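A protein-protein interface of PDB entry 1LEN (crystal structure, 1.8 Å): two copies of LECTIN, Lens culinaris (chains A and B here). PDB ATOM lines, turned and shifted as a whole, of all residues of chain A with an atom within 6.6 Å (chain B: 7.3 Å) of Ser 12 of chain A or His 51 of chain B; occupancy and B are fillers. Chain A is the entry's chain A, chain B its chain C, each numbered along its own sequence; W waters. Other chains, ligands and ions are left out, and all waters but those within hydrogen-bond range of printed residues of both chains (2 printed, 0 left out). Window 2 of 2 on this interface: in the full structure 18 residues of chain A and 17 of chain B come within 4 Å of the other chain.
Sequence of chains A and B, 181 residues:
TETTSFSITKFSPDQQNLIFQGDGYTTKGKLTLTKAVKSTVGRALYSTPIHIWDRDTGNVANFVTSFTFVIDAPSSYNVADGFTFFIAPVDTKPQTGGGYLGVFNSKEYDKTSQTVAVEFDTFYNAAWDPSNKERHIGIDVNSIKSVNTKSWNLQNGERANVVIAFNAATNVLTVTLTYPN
N of Ser 12 of chain A lies within hydrogen-bond range of OE1 of Gln 15 of chain A (2.9 Å).
OG1 of Thr 26 of chain A lies within hydrogen-bond range of O of Ser 12 of chain A (2.7 Å).
The side-chain amide nitrogen (NE2) of Gln 16 of chain A lies within hydrogen-bond range of the side-chain carboxylate (OD2) of Asp 14 of chain A (3.0 Å).
OD1 of Asn 17 of chain A is in hydrogen-bond range of NE2 of Gln 15 of chain A, at 2.7 Å.
The side-chain carboxylate (OE1) of Glu 2 of chain B is in hydrogen-bond range of a ring nitrogen (ND1) of His 51 of chain B.
O of Trp 53 of chain B sits close to NE2 of His 51 of chain B (3.4 Å).
Water W1 lies within hydrogen-bond range of the backbone carbonyl oxygen of Pro 49 of chain B (2.7 Å), the side-chain amide nitrogen of Asn 17 of chain A (3.0 Å) and the side-chain hydroxyl of Thr 4 of chain B (3.3 Å).
Water W2 lies within hydrogen-bond range of the side-chain hydroxyl (OG1) of Thr 4 of chain B, the side-chain carboxylate (OE2) of Glu 2 of chain B and the side-chain amide nitrogen (ND2) of Asn 17 of chain A.
The side-chain amide nitrogen (NE2) of Gln 15 of chain A lies within hydrogen-bond range of the side-chain carboxylate (OE2) of Glu 2 of chain B (3.3 Å).
OE2 of Glu 2 of chain B sits at hydrogen-bond distance from ND2 of Asn 17 of chain A (3.2 Å).
No position is printed for both chains.
Printed residues of chain B that touch a printed residue of chain A: Glu 2, Pro 49 and His 51.
Hydrophobic or aromatic side chains of chain B within 4 Å of the printed part of chain A: Pro 49 and His 51.
Along chain B the printed residues that touch a printed residue of chain A span positions 2 to 51.
Printed residues of chain A that touch a printed residue of chain B: Ser 12, Gln 15, Gln 16 and Asn 17.
Among the printed residues, pairs that only touch across the chains: Ser 12 of chain A with His 51 of chain B (3.4 Å), Gln 16 of chain A with Pro 49 of chain B (3.7 Å) and Asn 17 of chain A with Pro 49 of chain B (3.96 Å).
Ser 12 of chain A touches just one residue of chain B: His 51.
Of the printed residues of chain A, Glu 2 of chain B touches Gln 15 (3.3 Å) and Asn 17 (3.2 Å).
Of the printed residues of chain A, Pro 49 of chain B touches Gln 16 (3.7 Å) and Asn 17 (3.96 Å).
Printed residues of chain A within 4 Å of His 51 of chain B: Ser 12 (3.4 Å).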
ATOM      1  N   ILE A   8      19.132  17.450  18.485  1.00  0.00           N
ATOM      2  CA  ILE A   8      19.181  18.640  19.323  1.00  0.00           C
ATOM      3  C   ILE A   8      18.323  18.400  20.570  1.00  0.00           C
ATOM      4  O   ILE A   8      17.144  18.395  20.281  1.00  0.00           O
ATOM      5  CB  ILE A   8      18.727  19.883  18.627  1.00  0.00           C
ATOM      6  CG1 ILE A   8      19.493  20.140  17.354  1.00  0.00           C
ATOM      7  CG2 ILE A   8      18.804  21.077  19.579  1.00  0.00           C
ATOM      8  CD1 ILE A   8      19.261  21.476  16.715  1.00  0.00           C
ATOM      9  N   LYS A  10      18.523  20.213  23.351  1.00  0.00           N
ATOM     10  CA  LYS A  10      18.313  21.476  24.062  1.00  0.00           C
ATOM     11  C   LYS A  10      18.712  22.624  23.139  1.00  0.00           C
ATOM     12  O   LYS A  10      19.833  22.461  22.683  1.00  0.00           O
ATOM     13  CB  LYS A  10      19.167  21.509  25.325  1.00  0.00           C
ATOM     14  CG  LYS A  10      18.295  22.146  26.396  1.00  0.00           C
ATOM     15  CD  LYS A  10      18.876  22.126  27.771  1.00  0.00           C
ATOM     16  CE  LYS A  10      18.901  23.500  28.414  1.00  0.00           C
ATOM     17  NZ  LYS A  10      17.786  23.704  29.354  1.00  0.00           N
ATOM     18  N   PHE A  11      17.893  23.592  22.885  1.00  0.00           N
ATOM     19  CA  PHE A  11      18.120  24.715  22.007  1.00  0.00           C
ATOM     20  C   PHE A  11      18.801  25.882  22.697  1.00  0.00           C
ATOM     21  O   PHE A  11      18.399  26.361  23.745  1.00  0.00           O
ATOM     22  CB  PHE A  11      16.806  25.219  21.389  1.00  0.00           C
ATOM     23  CG  PHE A  11      16.154  24.164  20.514  1.00  0.00           C
ATOM     24  CD1 PHE A  11      15.332  23.184  21.045  1.00  0.00           C
ATOM     25  CD2 PHE A  11      16.373  24.190  19.140  1.00  0.00           C
ATOM     26  CE1 PHE A  11      14.700  22.185  20.294  1.00  0.00           C
ATOM     27  CE2 PHE A  11      15.744  23.242  18.380  1.00  0.00           C
ATOM     28  CZ  PHE A  11      14.925  22.253  18.923  1.00  0.00           C
ATOM     29  N   SER A  12      19.804  26.334  22.010  1.00  0.00           N
ATOM     30  CA  SER A  12      20.701  27.463  22.282  1.00  0.00           C
ATOM     31  C   SER A  12      19.966  28.763  21.893  1.00  0.00           C
ATOM     32  O   SER A  12      19.144  28.702  20.999  1.00  0.00           O
ATOM     33  CB  SER A  12      21.960  27.387  21.418  1.00  0.00           C
ATOM     34  OG  SER A  12      23.006  26.626  21.933  1.00  0.00           O
ATOM     35  N   PRO A  13      20.319  29.839  22.513  1.00  0.00           N
ATOM     36  CA  PRO A  13      19.728  31.159  22.221  1.00  0.00           C
ATOM     37  C   PRO A  13      20.159  31.615  20.833  1.00  0.00           C
ATOM     38  O   PRO A  13      19.439  32.370  20.168  1.00  0.00           O
ATOM     39  CB  PRO A  13      20.381  31.977  23.305  1.00  0.00           C
ATOM     40  CG  PRO A  13      21.412  31.127  24.007  1.00  0.00           C
ATOM     41  CD  PRO A  13      21.628  29.908  23.141  1.00  0.00           C
ATOM     42  N   ASP A  14      21.324  31.143  20.405  1.00  0.00           N
ATOM     43  CA  ASP A  14      21.914  31.362  19.108  1.00  0.00           C
ATOM     44  C   ASP A  14      22.184  30.051  18.392  1.00  0.00           C
ATOM     45  O   ASP A  14      23.238  29.466  18.316  1.00  0.00           O
ATOM     46  CB  ASP A  14      23.003  32.344  18.948  1.00  0.00           C
ATOM     47  CG  ASP A  14      23.076  32.881  17.496  1.00  0.00           C
ATOM     48  OD1 ASP A  14      22.060  33.021  16.794  1.00  0.00           O
ATOM     49  OD2 ASP A  14      24.184  33.185  17.029  1.00  0.00           O
ATOM     50  N   GLN A  15      21.015  29.645  17.893  1.00  0.00           N
ATOM     51  CA  GLN A  15      21.045  28.342  17.178  1.00  0.00           C
ATOM     52  C   GLN A  15      21.284  28.654  15.708  1.00  0.00           C
ATOM     53  O   GLN A  15      20.347  28.841  14.971  1.00  0.00           O
ATOM     54  CB  GLN A  15      19.726  27.629  17.397  1.00  0.00           C
ATOM     55  CG  GLN A  15      19.685  26.164  17.436  1.00  0.00           C
ATOM     56  CD  GLN A  15      20.692  25.359  18.163  1.00  0.00           C
ATOM     57  OE1 GLN A  15      20.888  25.421  19.448  1.00  0.00           O
ATOM     58  NE2 GLN A  15      21.417  24.469  17.446  1.00  0.00           N
ATOM     59  N   GLN A  16      22.546  28.767  15.348  1.00  0.00           N
ATOM     60  CA  GLN A  16      22.981  29.121  14.002  1.00  0.00           C
ATOM     61  C   GLN A  16      22.654  28.093  12.966  1.00  0.00           C
ATOM     62  O   GLN A  16      22.710  28.416  11.783  1.00  0.00           O
ATOM     63  CB  GLN A  16      24.459  29.510  13.961  1.00  0.00           C
ATOM     64  CG  GLN A  16      24.681  30.957  13.542  1.00  0.00           C
ATOM     65  CD  GLN A  16      25.683  31.652  14.461  1.00  0.00           C
ATOM     66  OE1 GLN A  16      26.428  30.911  15.252  1.00  0.00           O
ATOM     67  NE2 GLN A  16      25.808  32.988  14.529  1.00  0.00           N
ATOM     68  N   ASN A  17      22.323  26.856  13.323  1.00  0.00           N
ATOM     69  CA  ASN A  17      22.007  25.899  12.267  1.00  0.00           C
ATOM     70  C   ASN A  17      20.522  25.867  11.973  1.00  0.00           C
ATOM     71  O   ASN A  17      20.102  24.963  11.276  1.00  0.00           O
ATOM     72  CB  ASN A  17      22.554  24.529  12.553  1.00  0.00           C
ATOM     73  CG  ASN A  17      22.198  24.001  13.915  1.00  0.00           C
ATOM     74  OD1 ASN A  17      21.472  24.702  14.730  1.00  0.00           O
ATOM     75  ND2 ASN A  17      22.613  22.820  14.328  1.00  0.00           N
ATOM     76  N   PHE A  20      14.950  31.015  11.188  1.00  0.00           N
ATOM     77  CA  PHE A  20      13.699  31.392  11.851  1.00  0.00           C
ATOM     78  C   PHE A  20      12.890  32.328  10.974  1.00  0.00           C
ATOM     79  O   PHE A  20      13.465  33.218  10.380  1.00  0.00           O
ATOM     80  CB  PHE A  20      13.995  32.106  13.175  1.00  0.00           C
ATOM     81  CG  PHE A  20      14.608  31.123  14.196  1.00  0.00           C
ATOM     82  CD1 PHE A  20      13.780  30.235  14.798  1.00  0.00           C
ATOM     83  CD2 PHE A  20      15.959  31.237  14.459  1.00  0.00           C
ATOM     84  CE1 PHE A  20      14.409  29.455  15.685  1.00  0.00           C
ATOM     85  CE2 PHE A  20      16.576  30.400  15.365  1.00  0.00           C
ATOM     86  CZ  PHE A  20      15.743  29.498  15.985  1.00  0.00           C
ATOM     87  N   TYR A  25      11.667  31.733  17.648  1.00  0.00           N
ATOM     88  CA  TYR A  25      12.898  32.124  18.351  1.00  0.00           C
ATOM     89  C   TYR A  25      13.315  31.030  19.316  1.00  0.00           C
ATOM     90  O   TYR A  25      12.472  30.157  19.533  1.00  0.00           O
ATOM     91  CB  TYR A  25      12.774  33.458  19.048  1.00  0.00           C
ATOM     92  CG  TYR A  25      11.845  33.572  20.258  1.00  0.00           C
ATOM     93  CD1 TYR A  25      10.446  33.520  20.122  1.00  0.00           C
ATOM     94  CD2 TYR A  25      12.357  33.740  21.549  1.00  0.00           C
ATOM     95  CE1 TYR A  25       9.603  33.599  21.224  1.00  0.00           C
ATOM     96  CE2 TYR A  25      11.516  33.827  22.653  1.00  0.00           C
ATOM     97  CZ  TYR A  25      10.132  33.752  22.500  1.00  0.00           C
ATOM     98  OH  TYR A  25       9.320  33.831  23.611  1.00  0.00           O
ATOM     99  N   THR A  26      14.495  31.011  19.874  1.00  0.00           N
ATOM    100  CA  THR A  26      14.850  29.994  20.877  1.00  0.00           C
ATOM    101  C   THR A  26      14.919  30.681  22.247  1.00  0.00           C
ATOM    102  O   THR A  26      15.316  31.825  22.354  1.00  0.00           O
ATOM    103  CB  THR A  26      16.168  29.325  20.587  1.00  0.00           C
ATOM    104  OG1 THR A  26      17.117  30.256  20.080  1.00  0.00           O
ATOM    105  CG2 THR A  26      15.971  28.210  19.597  1.00  0.00           C
ATOM    106  N   THR A  27      14.521  29.956  23.241  1.00  0.00           N
ATOM    107  CA  THR A  27      14.546  30.586  24.582  1.00  0.00           C
ATOM    108  C   THR A  27      14.380  29.492  25.634  1.00  0.00           C
ATOM    109  O   THR A  27      13.456  28.688  25.527  1.00  0.00           O
ATOM    110  CB  THR A  27      13.322  31.515  24.679  1.00  0.00           C
ATOM    111  OG1 THR A  27      13.326  32.161  25.952  1.00  0.00           O
ATOM    112  CG2 THR A  27      12.080  30.662  24.599  1.00  0.00           C
ATOM    113  N   GLY A  29      16.279  26.913  26.305  1.00  0.00           N
ATOM    114  CA  GLY A  29      16.410  25.483  25.949  1.00  0.00           C
ATOM    115  C   GLY A  29      15.324  25.019  25.009  1.00  0.00           C
ATOM    116  O   GLY A  29      15.375  23.906  24.530  1.00  0.00           O
ATOM    117  N   LYS A  30      14.358  25.881  24.725  1.00  0.00           N
ATOM    118  CA  LYS A  30      13.280  25.509  23.853  1.00  0.00           C
ATOM    119  C   LYS A  30      13.123  26.375  22.644  1.00  0.00           C
ATOM    120  O   LYS A  30      13.563  27.478  22.600  1.00  0.00           O
ATOM    121  CB  LYS A  30      11.990  25.220  24.533  1.00  0.00           C
ATOM    122  CG  LYS A  30      11.632  25.752  25.836  1.00  0.00           C
ATOM    123  CD  LYS A  30      10.444  26.701  25.725  1.00  0.00           C
ATOM    124  CE  LYS A  30       9.849  26.955  27.102  1.00  0.00           C
ATOM    125  NZ  LYS A  30       9.199  28.287  27.114  1.00  0.00           N
ATOM    126  N   GLU B   2      23.937  17.851  21.469  1.00  0.00           N
ATOM    127  CA  GLU B   2      23.725  18.270  20.072  1.00  0.00           C
ATOM    128  C   GLU B   2      24.603  17.466  19.153  1.00  0.00           C
ATOM    129  O   GLU B   2      25.818  17.469  19.277  1.00  0.00           O
ATOM    130  CB  GLU B   2      23.941  19.758  19.948  1.00  0.00           C
ATOM    131  CG  GLU B   2      23.564  20.297  18.644  1.00  0.00           C
ATOM    132  CD  GLU B   2      23.674  21.802  18.495  1.00  0.00           C
ATOM    133  OE1 GLU B   2      23.670  22.591  19.450  1.00  0.00           O
ATOM    134  OE2 GLU B   2      23.766  22.116  17.282  1.00  0.00           O
ATOM    135  N   THR B   4      25.810  15.878  15.137  1.00  0.00           N
ATOM    136  CA  THR B   4      25.671  16.122  13.688  1.00  0.00           C
ATOM    137  C   THR B   4      26.502  15.068  12.942  1.00  0.00           C
ATOM    138  O   THR B   4      27.609  14.815  13.388  1.00  0.00           O
ATOM    139  CB  THR B   4      26.115  17.511  13.311  1.00  0.00           C
ATOM    140  OG1 THR B   4      25.062  18.467  13.460  1.00  0.00           O
ATOM    141  CG2 THR B   4      26.538  17.546  11.867  1.00  0.00           C
ATOM    142  N   THR B  48      26.252  23.424   6.708  1.00  0.00           N
ATOM    143  CA  THR B  48      25.709  23.596   8.061  1.00  0.00           C
ATOM    144  C   THR B  48      26.729  24.200   9.022  1.00  0.00           C
ATOM    145  O   THR B  48      27.854  23.707   9.149  1.00  0.00           O
ATOM    146  CB  THR B  48      25.368  22.206   8.620  1.00  0.00           C
ATOM    147  OG1 THR B  48      24.957  21.340   7.625  1.00  0.00           O
ATOM    148  CG2 THR B  48      24.461  22.279   9.778  1.00  0.00           C
ATOM    149  N   PRO B  49      26.377  25.178   9.839  1.00  0.00           N
ATOM    150  CA  PRO B  49      27.398  25.625  10.831  1.00  0.00           C
ATOM    151  C   PRO B  49      27.489  24.568  11.907  1.00  0.00           C
ATOM    152  O   PRO B  49      26.458  23.964  12.189  1.00  0.00           O
ATOM    153  CB  PRO B  49      26.750  26.883  11.341  1.00  0.00           C
ATOM    154  CG  PRO B  49      25.865  27.402  10.231  1.00  0.00           C
ATOM    155  CD  PRO B  49      25.314  26.128   9.599  1.00  0.00           C
ATOM    156  N   ILE B  50      28.648  24.253  12.469  1.00  0.00           N
ATOM    157  CA  ILE B  50      28.711  23.199  13.498  1.00  0.00           C
ATOM    158  C   ILE B  50      29.010  23.815  14.861  1.00  0.00           C
ATOM    159  O   ILE B  50      29.837  24.716  14.903  1.00  0.00           O
ATOM    160  CB  ILE B  50      29.757  22.165  13.149  1.00  0.00           C
ATOM    161  CG1 ILE B  50      29.323  21.366  11.908  1.00  0.00           C
ATOM    162  CG2 ILE B  50      30.059  21.231  14.302  1.00  0.00           C
ATOM    163  CD1 ILE B  50      30.477  21.116  10.982  1.00  0.00           C
ATOM    164  N   HIS B  51      28.323  23.356  15.855  1.00  0.00           N
ATOM    165  CA  HIS B  51      28.471  23.809  17.260  1.00  0.00           C
ATOM    166  C   HIS B  51      29.635  22.989  17.875  1.00  0.00           C
ATOM    167  O   HIS B  51      29.452  21.846  18.215  1.00  0.00           O
ATOM    168  CB  HIS B  51      27.207  23.485  18.034  1.00  0.00           C
ATOM    169  CG  HIS B  51      26.947  24.490  19.124  1.00  0.00           C
ATOM    170  ND1 HIS B  51      25.841  24.442  19.975  1.00  0.00           N
ATOM    171  CD2 HIS B  51      27.760  25.540  19.463  1.00  0.00           C
ATOM    172  CE1 HIS B  51      25.984  25.533  20.825  1.00  0.00           C
ATOM    173  NE2 HIS B  51      27.129  26.185  20.487  1.00  0.00           N
ATOM    174  N   ILE B  52      30.780  23.655  17.935  1.00  0.00           N
ATOM    175  CA  ILE B  52      32.084  23.209  18.364  1.00  0.00           C
ATOM    176  C   ILE B  52      32.357  23.237  19.826  1.00  0.00           C
ATOM    177  O   ILE B  52      32.965  22.300  20.397  1.00  0.00           O
ATOM    178  CB  ILE B  52      33.188  23.494  17.440  1.00  0.00           C
ATOM    179  CG1 ILE B  52      34.104  22.364  17.082  1.00  0.00           C
ATOM    180  CG2 ILE B  52      33.846  24.834  17.541  1.00  0.00           C
ATOM    181  CD1 ILE B  52      33.621  21.256  16.213  1.00  0.00           C
ATOM    182  N   TRP B  53      31.946  24.269  20.535  1.00  0.00           N
ATOM    183  CA  TRP B  53      32.052  24.463  21.970  1.00  0.00           C
ATOM    184  C   TRP B  53      30.919  25.324  22.467  1.00  0.00           C
ATOM    185  O   TRP B  53      30.367  26.035  21.618  1.00  0.00           O
ATOM    186  CB  TRP B  53      33.383  24.885  22.469  1.00  0.00           C
ATOM    187  CG  TRP B  53      33.884  26.226  22.038  1.00  0.00           C
ATOM    188  CD1 TRP B  53      34.455  26.564  20.858  1.00  0.00           C
ATOM    189  CD2 TRP B  53      33.832  27.371  22.827  1.00  0.00           C
ATOM    190  NE1 TRP B  53      34.769  27.941  20.906  1.00  0.00           N
ATOM    191  CE2 TRP B  53      34.387  28.398  22.086  1.00  0.00           C
ATOM    192  CE3 TRP B  53      33.350  27.596  24.125  1.00  0.00           C
ATOM    193  CZ2 TRP B  53      34.482  29.647  22.571  1.00  0.00           C
ATOM    194  CZ3 TRP B  53      33.457  28.883  24.614  1.00  0.00           C
ATOM    195  CH2 TRP B  53      34.016  29.887  23.850  1.00  0.00           C
ATOM    196  N   ASP B  54      30.599  25.231  23.721  1.00  0.00           N
ATOM    197  CA  ASP B  54      29.459  26.019  24.272  1.00  0.00           C
ATOM    198  C   ASP B  54      29.978  26.981  25.331  1.00  0.00           C
ATOM    199  O   ASP B  54      30.508  26.502  26.341  1.00  0.00           O
ATOM    200  CB  ASP B  54      28.508  25.011  24.953  1.00  0.00           C
ATOM    201  CG  ASP B  54      27.236  25.707  25.416  1.00  0.00           C
ATOM    202  OD1 ASP B  54      27.019  26.864  25.069  1.00  0.00           O
ATOM    203  OD2 ASP B  54      26.446  25.042  26.094  1.00  0.00           O
ATOM    204  N   ARG B  55      29.907  28.266  25.142  1.00  0.00           N
ATOM    205  CA  ARG B  55      30.423  29.275  26.068  1.00  0.00           C
ATOM    206  C   ARG B  55      29.850  29.112  27.469  1.00  0.00           C
ATOM    207  O   ARG B  55      30.603  29.291  28.431  1.00  0.00           O
ATOM    208  CB  ARG B  55      30.148  30.686  25.569  1.00  0.00           C
ATOM    209  CG  ARG B  55      31.336  31.584  25.909  1.00  0.00           C
ATOM    210  CD  ARG B  55      31.458  32.739  24.901  1.00  0.00           C
ATOM    211  NE  ARG B  55      32.596  33.587  25.294  1.00  0.00           N
ATOM    212  CZ  ARG B  55      33.361  34.189  24.351  1.00  0.00           C
ATOM    213  NH1 ARG B  55      33.090  34.018  23.056  1.00  0.00           N
ATOM    214  NH2 ARG B  55      34.400  34.957  24.680  1.00  0.00           N
ATOM    215  N   ASP B  56      28.613  28.790  27.543  1.00  0.00           N
ATOM    216  CA  ASP B  56      27.707  28.544  28.664  1.00  0.00           C
ATOM    217  C   ASP B  56      28.206  27.421  29.546  1.00  0.00           C
ATOM    218  O   ASP B  56      28.427  27.522  30.735  1.00  0.00           O
ATOM    219  CB  ASP B  56      26.310  28.157  28.137  1.00  0.00           C
ATOM    220  CG  ASP B  56      25.505  29.432  27.848  1.00  0.00           C
ATOM    221  OD1 ASP B  56      25.931  30.356  27.145  1.00  0.00           O
ATOM    222  OD2 ASP B  56      24.400  29.448  28.399  1.00  0.00           O
ATOM    223  N   ASN B  59      31.619  23.237  27.506  1.00  0.00           N
ATOM    224  CA  ASN B  59      31.845  21.953  26.810  1.00  0.00           C
ATOM    225  C   ASN B  59      32.422  22.209  25.410  1.00  0.00           C
ATOM    226  O   ASN B  59      32.140  23.196  24.731  1.00  0.00           O
ATOM    227  CB  ASN B  59      30.480  21.265  26.604  1.00  0.00           C
ATOM    228  CG  ASN B  59      29.926  20.813  27.949  1.00  0.00           C
ATOM    229  OD1 ASN B  59      30.768  20.453  28.889  1.00  0.00           O
ATOM    230  ND2 ASN B  59      28.625  20.818  28.116  1.00  0.00           N
ATOM    231  N   VAL B  60      33.238  21.277  25.024  1.00  0.00           N
ATOM    232  CA  VAL B  60      33.889  21.226  23.708  1.00  0.00           C
ATOM    233  C   VAL B  60      33.472  19.941  23.021  1.00  0.00           C
ATOM    234  O   VAL B  60      33.278  18.892  23.676  1.00  0.00           O
ATOM    235  CB  VAL B  60      35.392  21.381  23.823  1.00  0.00           C
ATOM    236  CG1 VAL B  60      36.079  21.626  22.485  1.00  0.00           C
ATOM    237  CG2 VAL B  60      35.790  22.594  24.721  1.00  0.00           C
ATOM    238  N   ALA B  61      33.253  19.951  21.723  1.00  0.00           N
ATOM    239  CA  ALA B  61      32.791  18.765  21.026  1.00  0.00           C
ATOM    240  C   ALA B  61      33.881  17.763  20.741  1.00  0.00           C
ATOM    241  O   ALA B  61      35.020  18.121  20.583  1.00  0.00           O
ATOM    242  CB  ALA B  61      32.175  19.153  19.677  1.00  0.00           C
ATOM    243  N   ASN B  62      33.495  16.501  20.691  1.00  0.00           N
ATOM    244  CA  ASN B  62      34.350  15.403  20.241  1.00  0.00           C
ATOM    245  C   ASN B  62      34.034  15.265  18.709  1.00  0.00           C
ATOM    246  O   ASN B  62      32.845  15.464  18.404  1.00  0.00           O
ATOM    247  CB  ASN B  62      33.992  14.069  20.861  1.00  0.00           C
ATOM    248  CG  ASN B  62      34.315  13.917  22.329  1.00  0.00           C
ATOM    249  OD1 ASN B  62      33.450  13.433  23.183  1.00  0.00           O
ATOM    250  ND2 ASN B  62      35.489  14.275  22.746  1.00  0.00           N
HETATM  251  O   HOH W   1      25.102  21.754  12.936  1.00  0.00           O
HETATM  252  O   HOH W   2      22.769  19.524  15.409  1.00  0.00           O
